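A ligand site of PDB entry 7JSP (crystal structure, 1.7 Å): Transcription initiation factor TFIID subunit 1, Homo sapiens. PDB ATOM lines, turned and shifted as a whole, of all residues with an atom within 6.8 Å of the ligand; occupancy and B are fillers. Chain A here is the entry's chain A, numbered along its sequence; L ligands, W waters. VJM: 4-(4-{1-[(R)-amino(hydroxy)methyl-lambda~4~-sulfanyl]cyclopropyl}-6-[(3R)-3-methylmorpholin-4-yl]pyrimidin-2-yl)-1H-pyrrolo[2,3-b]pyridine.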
ATOM      1  N   TRP A  28      23.394  24.260   4.736  1.00  0.00           N
ATOM      2  CA  TRP A  28      22.803  25.288   3.876  1.00  0.00           C
ATOM      3  C   TRP A  28      23.190  25.156   2.407  1.00  0.00           C
ATOM      4  O   TRP A  28      22.379  25.537   1.540  1.00  0.00           O
ATOM      5  CB  TRP A  28      23.172  26.701   4.387  1.00  0.00           C
ATOM      6  CG  TRP A  28      24.642  26.949   4.410  1.00  0.00           C
ATOM      7  CD1 TRP A  28      25.498  26.772   5.474  1.00  0.00           C
ATOM      8  CD2 TRP A  28      25.447  27.389   3.318  1.00  0.00           C
ATOM      9  NE1 TRP A  28      26.773  27.079   5.088  1.00  0.00           N
ATOM     10  CE2 TRP A  28      26.776  27.454   3.774  1.00  0.00           C
ATOM     11  CE3 TRP A  28      25.171  27.733   1.989  1.00  0.00           C
ATOM     12  CZ2 TRP A  28      27.822  27.846   2.960  1.00  0.00           C
ATOM     13  CZ3 TRP A  28      26.217  28.125   1.175  1.00  0.00           C
ATOM     14  CH2 TRP A  28      27.529  28.175   1.659  1.00  0.00           C
ATOM     15  N   PRO A  29      24.389  24.657   2.042  1.00  0.00           N
ATOM     16  CA  PRO A  29      24.720  24.636   0.604  1.00  0.00           C
ATOM     17  C   PRO A  29      23.788  23.746  -0.182  1.00  0.00           C
ATOM     18  O   PRO A  29      23.693  23.893  -1.414  1.00  0.00           O
ATOM     19  CB  PRO A  29      26.158  24.113   0.584  1.00  0.00           C
ATOM     20  CG  PRO A  29      26.693  24.360   1.958  1.00  0.00           C
ATOM     21  CD  PRO A  29      25.512  24.141   2.837  1.00  0.00           C
ATOM     22  N   PHE A  30      23.099  22.820   0.478  1.00  0.00           N
ATOM     23  CA  PHE A  30      22.287  21.804  -0.164  1.00  0.00           C
ATOM     24  C   PHE A  30      20.808  21.990   0.050  1.00  0.00           C
ATOM     25  O   PHE A  30      20.011  21.173  -0.417  1.00  0.00           O
ATOM     26  CB  PHE A  30      22.743  20.426   0.353  1.00  0.00           C
ATOM     27  CG  PHE A  30      24.212  20.249   0.286  1.00  0.00           C
ATOM     28  CD1 PHE A  30      24.843  20.055  -0.921  1.00  0.00           C
ATOM     29  CD2 PHE A  30      24.983  20.309   1.440  1.00  0.00           C
ATOM     30  CE1 PHE A  30      26.208  19.899  -0.993  1.00  0.00           C
ATOM     31  CE2 PHE A  30      26.356  20.168   1.363  1.00  0.00           C
ATOM     32  CZ  PHE A  30      26.960  19.951   0.169  1.00  0.00           C
ATOM     33  N   HIS A  31      20.395  23.092   0.690  1.00  0.00           N
ATOM     34  CA  HIS A  31      18.979  23.334   0.946  1.00  0.00           C
ATOM     35  C   HIS A  31      18.211  23.815  -0.274  1.00  0.00           C
ATOM     36  O   HIS A  31      16.980  23.656  -0.298  1.00  0.00           O
ATOM     37  CB  HIS A  31      18.826  24.353   2.068  1.00  0.00           C
ATOM     38  CG  HIS A  31      19.100  23.812   3.441  1.00  0.00           C
ATOM     39  ND1 HIS A  31      18.603  24.403   4.573  1.00  0.00           N
ATOM     40  CD2 HIS A  31      19.832  22.750   3.859  1.00  0.00           C
ATOM     41  CE1 HIS A  31      19.014  23.733   5.638  1.00  0.00           C
ATOM     42  NE2 HIS A  31      19.759  22.728   5.225  1.00  0.00           N
ATOM     43  N   HIS A  32      18.866  24.388  -1.264  1.00  0.00           N
ATOM     44  CA  HIS A  32      18.197  25.022  -2.402  1.00  0.00           C
ATOM     45  C   HIS A  32      19.074  24.803  -3.628  1.00  0.00           C
ATOM     46  O   HIS A  32      20.260  24.499  -3.500  1.00  0.00           O
ATOM     47  CB  HIS A  32      17.993  26.536  -2.165  1.00  0.00           C
ATOM     48  CG  HIS A  32      17.213  26.855  -0.935  1.00  0.00           C
ATOM     49  ND1 HIS A  32      15.837  26.737  -0.874  1.00  0.00           N
ATOM     50  CD2 HIS A  32      17.610  27.284   0.289  1.00  0.00           C
ATOM     51  CE1 HIS A  32      15.427  27.082   0.339  1.00  0.00           C
ATOM     52  NE2 HIS A  32      16.477  27.420   1.059  1.00  0.00           N
ATOM     53  N   PRO A  33      18.510  24.980  -4.824  1.00  0.00           N
ATOM     54  CA  PRO A  33      19.337  24.967  -6.031  1.00  0.00           C
ATOM     55  C   PRO A  33      20.394  26.061  -5.975  1.00  0.00           C
ATOM     56  O   PRO A  33      20.164  27.146  -5.411  1.00  0.00           O
ATOM     57  CB  PRO A  33      18.331  25.210  -7.165  1.00  0.00           C
ATOM     58  CG  PRO A  33      16.999  24.885  -6.585  1.00  0.00           C
ATOM     59  CD  PRO A  33      17.088  25.220  -5.127  1.00  0.00           C
ATOM     60  N   VAL A  34      21.561  25.771  -6.541  1.00  0.00           N
ATOM     61  CA  VAL A  34      22.585  26.789  -6.692  1.00  0.00           C
ATOM     62  C   VAL A  34      22.077  27.876  -7.609  1.00  0.00           C
ATOM     63  O   VAL A  34      21.490  27.590  -8.668  1.00  0.00           O
ATOM     64  CB  VAL A  34      23.882  26.161  -7.231  1.00  0.00           C
ATOM     65  CG1 VAL A  34      24.885  27.238  -7.617  1.00  0.00           C
ATOM     66  CG2 VAL A  34      24.476  25.189  -6.226  1.00  0.00           C
ATOM     67  N   ASN A  35      22.295  29.135  -7.220  1.00  0.00           N
ATOM     68  CA  ASN A  35      21.939  30.290  -8.019  1.00  0.00           C
ATOM     69  C   ASN A  35      23.006  30.521  -9.081  1.00  0.00           C
ATOM     70  O   ASN A  35      24.176  30.770  -8.762  1.00  0.00           O
ATOM     71  CB  ASN A  35      21.804  31.515  -7.126  1.00  0.00           C
ATOM     72  CG  ASN A  35      21.269  32.734  -7.828  1.00  0.00           C
ATOM     73  OD1 ASN A  35      21.365  32.886  -9.061  1.00  0.00           O
ATOM     74  ND2 ASN A  35      20.674  33.634  -7.066  1.00  0.00           N
ATOM     75  N   LYS A  36      22.596  30.468 -10.357  1.00  0.00           N
ATOM     76  CA  LYS A  36      23.540  30.634 -11.461  1.00  0.00           C
ATOM     77  C   LYS A  36      24.192  32.007 -11.459  1.00  0.00           C
ATOM     78  O   LYS A  36      25.304  32.176 -12.004  1.00  0.00           O
ATOM     79  CB  LYS A  36      22.801  30.401 -12.781  1.00  0.00           C
ATOM     80  CG  LYS A  36      23.688  30.251 -14.010  1.00  0.00           C
ATOM     81  CD  LYS A  36      22.845  29.979 -15.252  1.00  0.00           C
ATOM     82  CE  LYS A  36      23.406  28.818 -16.061  1.00  0.00           C
ATOM     83  NZ  LYS A  36      22.452  28.348 -17.120  1.00  0.00           N
ATOM     84  N   PHE A  38      25.222  33.553  -8.822  1.00  0.00           N
ATOM     85  CA  PHE A  38      26.263  33.487  -7.799  1.00  0.00           C
ATOM     86  C   PHE A  38      27.395  32.534  -8.207  1.00  0.00           C
ATOM     87  O   PHE A  38      28.567  32.834  -7.975  1.00  0.00           O
ATOM     88  CB  PHE A  38      25.676  33.029  -6.478  1.00  0.00           C
ATOM     89  CG  PHE A  38      24.629  33.965  -5.909  1.00  0.00           C
ATOM     90  CD1 PHE A  38      24.568  35.283  -6.295  1.00  0.00           C
ATOM     91  CD2 PHE A  38      23.715  33.506  -4.981  1.00  0.00           C
ATOM     92  CE1 PHE A  38      23.614  36.131  -5.772  1.00  0.00           C
ATOM     93  CE2 PHE A  38      22.762  34.350  -4.448  1.00  0.00           C
ATOM     94  CZ  PHE A  38      22.710  35.674  -4.844  1.00  0.00           C
ATOM     95  N   VAL A  39      27.064  31.407  -8.825  1.00  0.00           N
ATOM     96  CA  VAL A  39      28.053  30.399  -9.181  1.00  0.00           C
ATOM     97  C   VAL A  39      27.830  30.013 -10.640  1.00  0.00           C
ATOM     98  O   VAL A  39      27.348  28.910 -10.918  1.00  0.00           O
ATOM     99  CB  VAL A  39      27.956  29.171  -8.260  1.00  0.00           C
ATOM    100  CG1 VAL A  39      29.199  28.307  -8.417  1.00  0.00           C
ATOM    101  CG2 VAL A  39      27.749  29.600  -6.804  1.00  0.00           C
ATOM    102  N   TYR A  42      28.755  26.548 -11.993  1.00  0.00           N
ATOM    103  CA  TYR A  42      28.197  25.335 -11.416  1.00  0.00           C
ATOM    104  C   TYR A  42      27.466  24.504 -12.465  1.00  0.00           C
ATOM    105  O   TYR A  42      27.629  23.285 -12.535  1.00  0.00           O
ATOM    106  CB  TYR A  42      27.252  25.676 -10.284  1.00  0.00           C
ATOM    107  CG  TYR A  42      26.829  24.450  -9.492  1.00  0.00           C
ATOM    108  CD1 TYR A  42      27.688  23.879  -8.581  1.00  0.00           C
ATOM    109  CD2 TYR A  42      25.574  23.887  -9.681  1.00  0.00           C
ATOM    110  CE1 TYR A  42      27.309  22.769  -7.861  1.00  0.00           C
ATOM    111  CE2 TYR A  42      25.198  22.755  -8.960  1.00  0.00           C
ATOM    112  CZ  TYR A  42      26.073  22.213  -8.060  1.00  0.00           C
ATOM    113  OH  TYR A  42      25.695  21.099  -7.330  1.00  0.00           O
ATOM    114  N   ASP A  51      18.979  19.005  -4.954  1.00  0.00           N
ATOM    115  CA  ASP A  51      19.058  19.681  -3.662  1.00  0.00           C
ATOM    116  C   ASP A  51      17.827  19.308  -2.848  1.00  0.00           C
ATOM    117  O   ASP A  51      16.877  18.702  -3.364  1.00  0.00           O
ATOM    118  CB  ASP A  51      19.153  21.193  -3.843  1.00  0.00           C
ATOM    119  CG  ASP A  51      17.903  21.766  -4.461  1.00  0.00           C
ATOM    120  OD1 ASP A  51      17.806  21.781  -5.719  1.00  0.00           O
ATOM    121  OD2 ASP A  51      16.988  22.140  -3.712  1.00  0.00           O
ATOM    122  N   ASN A  80      27.218  15.013  -6.722  1.00  0.00           N
ATOM    123  CA  ASN A  80      27.479  16.318  -7.325  1.00  0.00           C
ATOM    124  C   ASN A  80      28.475  17.119  -6.495  1.00  0.00           C
ATOM    125  O   ASN A  80      29.245  17.908  -7.047  1.00  0.00           O
ATOM    126  CB  ASN A  80      26.184  17.099  -7.463  1.00  0.00           C
ATOM    127  CG  ASN A  80      25.308  16.573  -8.596  1.00  0.00           C
ATOM    128  OD1 ASN A  80      25.780  15.885  -9.496  1.00  0.00           O
ATOM    129  ND2 ASN A  80      24.025  16.929  -8.552  1.00  0.00           N
ATOM    130  N   SER A  81      28.464  16.942  -5.180  1.00  0.00           N
ATOM    131  CA  SER A  81      29.469  17.608  -4.367  1.00  0.00           C
ATOM    132  C   SER A  81      30.846  17.001  -4.585  1.00  0.00           C
ATOM    133  O   SER A  81      31.845  17.711  -4.652  1.00  0.00           O
ATOM    134  CB  SER A  81      29.070  17.541  -2.876  1.00  0.00           C
ATOM    135  OG  SER A  81      29.983  18.279  -2.079  1.00  0.00           O
ATOM    136  N   TYR A  84      31.917  18.582  -7.988  1.00  0.00           N
ATOM    137  CA  TYR A  84      32.186  20.014  -8.063  1.00  0.00           C
ATOM    138  C   TYR A  84      33.203  20.470  -7.026  1.00  0.00           C
ATOM    139  O   TYR A  84      34.034  21.346  -7.313  1.00  0.00           O
ATOM    140  CB  TYR A  84      30.893  20.804  -7.880  1.00  0.00           C
ATOM    141  CG  TYR A  84      31.076  22.251  -8.304  1.00  0.00           C
ATOM    142  CD1 TYR A  84      31.073  22.592  -9.644  1.00  0.00           C
ATOM    143  CD2 TYR A  84      31.287  23.251  -7.372  1.00  0.00           C
ATOM    144  CE1 TYR A  84      31.266  23.897 -10.045  1.00  0.00           C
ATOM    145  CE2 TYR A  84      31.478  24.564  -7.769  1.00  0.00           C
ATOM    146  CZ  TYR A  84      31.470  24.879  -9.098  1.00  0.00           C
ATOM    147  OH  TYR A  84      31.663  26.178  -9.512  1.00  0.00           O
ATOM    148  N   ASN A  85      33.168  19.887  -5.824  1.00  0.00           N
ATOM    149  CA  ASN A  85      34.004  20.342  -4.719  1.00  0.00           C
ATOM    150  C   ASN A  85      35.161  19.408  -4.408  1.00  0.00           C
ATOM    151  O   ASN A  85      36.134  19.853  -3.800  1.00  0.00           O
ATOM    152  CB  ASN A  85      33.147  20.493  -3.459  1.00  0.00           C
ATOM    153  CG  ASN A  85      31.998  21.455  -3.660  1.00  0.00           C
ATOM    154  OD1 ASN A  85      32.204  22.599  -4.045  1.00  0.00           O
ATOM    155  ND2 ASN A  85      30.783  20.993  -3.402  1.00  0.00           N
ATOM    156  N   SER A  89      36.444  17.706   0.148  1.00  0.00           N
ATOM    157  CA  SER A  89      35.945  19.032   0.488  1.00  0.00           C
ATOM    158  C   SER A  89      35.039  18.958   1.717  1.00  0.00           C
ATOM    159  O   SER A  89      34.311  17.990   1.923  1.00  0.00           O
ATOM    160  CB  SER A  89      35.180  19.629  -0.693  1.00  0.00           C
ATOM    161  OG  SER A  89      34.507  20.827  -0.342  1.00  0.00           O
ATOM    162  N   TYR A  91      32.448  20.641   1.976  1.00  0.00           N
ATOM    163  CA  TYR A  91      31.113  20.535   1.414  1.00  0.00           C
ATOM    164  C   TYR A  91      30.704  19.074   1.290  1.00  0.00           C
ATOM    165  O   TYR A  91      29.547  18.713   1.588  1.00  0.00           O
ATOM    166  CB  TYR A  91      31.065  21.195   0.044  1.00  0.00           C
ATOM    167  CG  TYR A  91      31.061  22.710   0.069  1.00  0.00           C
ATOM    168  CD1 TYR A  91      30.007  23.409   0.622  1.00  0.00           C
ATOM    169  CD2 TYR A  91      32.103  23.428  -0.490  1.00  0.00           C
ATOM    170  CE1 TYR A  91      29.991  24.796   0.635  1.00  0.00           C
ATOM    171  CE2 TYR A  91      32.090  24.797  -0.485  1.00  0.00           C
ATOM    172  CZ  TYR A  91      31.039  25.475   0.091  1.00  0.00           C
ATOM    173  OH  TYR A  91      31.028  26.830   0.101  1.00  0.00           O
HETATM  174  C01 VJM L   1      28.771  25.627  -4.958  1.00  0.00           C
HETATM  175  C02 VJM L   1      28.707  25.343  -3.424  1.00  0.00           C
HETATM  176  C03 VJM L   1      29.456  24.010  -3.138  1.00  0.00           C
HETATM  177  C05 VJM L   1      27.393  22.753  -3.093  1.00  0.00           C
HETATM  178  C06 VJM L   1      26.598  24.076  -3.128  1.00  0.00           C
HETATM  179  C08 VJM L   1      26.626  26.517  -2.815  1.00  0.00           C
HETATM  180  C10 VJM L   1      26.685  28.941  -2.676  1.00  0.00           C
HETATM  181  C12 VJM L   1      24.590  27.841  -2.646  1.00  0.00           C
HETATM  182  C13 VJM L   1      25.223  26.586  -2.735  1.00  0.00           C
HETATM  183  C14 VJM L   1      23.136  27.984  -2.574  1.00  0.00           C
HETATM  184  C15 VJM L   1      22.208  26.770  -2.594  1.00  0.00           C
HETATM  185  C16 VJM L   1      22.367  27.596  -1.318  1.00  0.00           C
HETATM  186  C20 VJM L   1      22.769  30.925  -2.360  1.00  0.00           C
HETATM  187  C21 VJM L   1      27.389  30.167  -2.700  1.00  0.00           C
HETATM  188  C22 VJM L   1      28.716  30.315  -2.305  1.00  0.00           C
HETATM  189  C23 VJM L   1      29.626  29.428  -1.757  1.00  0.00           C
HETATM  190  C24 VJM L   1      30.798  30.152  -1.534  1.00  0.00           C
HETATM  191  C26 VJM L   1      29.355  31.560  -2.392  1.00  0.00           C
HETATM  192  C28 VJM L   1      27.445  32.555  -3.311  1.00  0.00           C
HETATM  193  C29 VJM L   1      26.764  31.321  -3.238  1.00  0.00           C
HETATM  194  N07 VJM L   1      27.351  25.323  -2.915  1.00  0.00           N
HETATM  195  N09 VJM L   1      27.294  27.717  -2.770  1.00  0.00           N
HETATM  196  N11 VJM L   1      25.342  28.946  -2.607  1.00  0.00           N
HETATM  197  N18 VJM L   1      20.926  29.301  -3.635  1.00  0.00           N
HETATM  198  N25 VJM L   1      30.580  31.435  -1.913  1.00  0.00           N
HETATM  199  N27 VJM L   1      28.727  32.661  -2.888  1.00  0.00           N
HETATM  200  O04 VJM L   1      28.725  22.869  -3.601  1.00  0.00           O
HETATM  201  O19 VJM L   1      23.442  29.706  -4.738  1.00  0.00           O
HETATM  202  S17 VJM L   1      22.539  29.480  -3.467  1.00  0.00           S
HETATM  203  O   HOH W   1      18.394  29.171  -5.972  1.00  0.00           O
HETATM  204  O   HOH W   2      19.141  30.501  -1.457  1.00  0.00           O
HETATM  205  O   HOH W   3      33.119  28.019  -1.029  1.00  0.00           O
HETATM  206  O   HOH W   4      27.563  20.326  -5.498  1.00  0.00           O
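An oxygen (O04) of the ligand lies within hydrogen-bond range of the side-chain amide nitrogen (ND2) of Asn 85, at 2.8 Å.
An oxygen (O19) of the ligand lies within hydrogen-bond range of the backbone NH of Asn 35 (2.8 Å).
N18 of the ligand is in hydrogen-bond range of O of Pro 33, 2.9 Å away.
The side-chain amide nitrogen of Asn 85 sits at hydrogen-bond distance from the side-chain hydroxyl of Ser 81, at 3.1 Å.
OG of Ser 89 lies close to N of Tyr 91 (3.1 Å).
Merely in contact with the ligand: His 32 (3.1 Å), Pro 29 (3.4 Å), Tyr 91 (3.5 Å), Trp 28 (3.5 Å), Val 34 (3.6 Å), Phe 38 (3.7 Å) and Phe 30 (3.7 Å).
Hydrophobic or aromatic side chains that line the ligand: Trp 28, Pro 29, Phe 30, Val 34, Phe 38 and Tyr 91.
Ten residues have an atom within 4 Å of the ligand: Trp 28, Pro 29, Phe 30, His 32, Pro 33, Val 34, Asn 35, Phe 38, Asn 85 and Tyr 91.
Along chain A the residues within 4 Å of the ligand span positions 28 to 91.
The nearest printed residue that does not touch the ligand is Tyr 84 (4.04 Å).
Water W4 lies within hydrogen-bond range of the side-chain hydroxyl of Tyr 42 (2.7 Å), the backbone carbonyl oxygen of Asn 80 (3.3 Å) and an oxygen (O04) of the ligand (3.4 Å).
Water W1 bridges the backbone carbonyl oxygen (O) of Pro 33 (2.7 Å) and a nitrogen (N18) of the ligand (3.4 Å).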
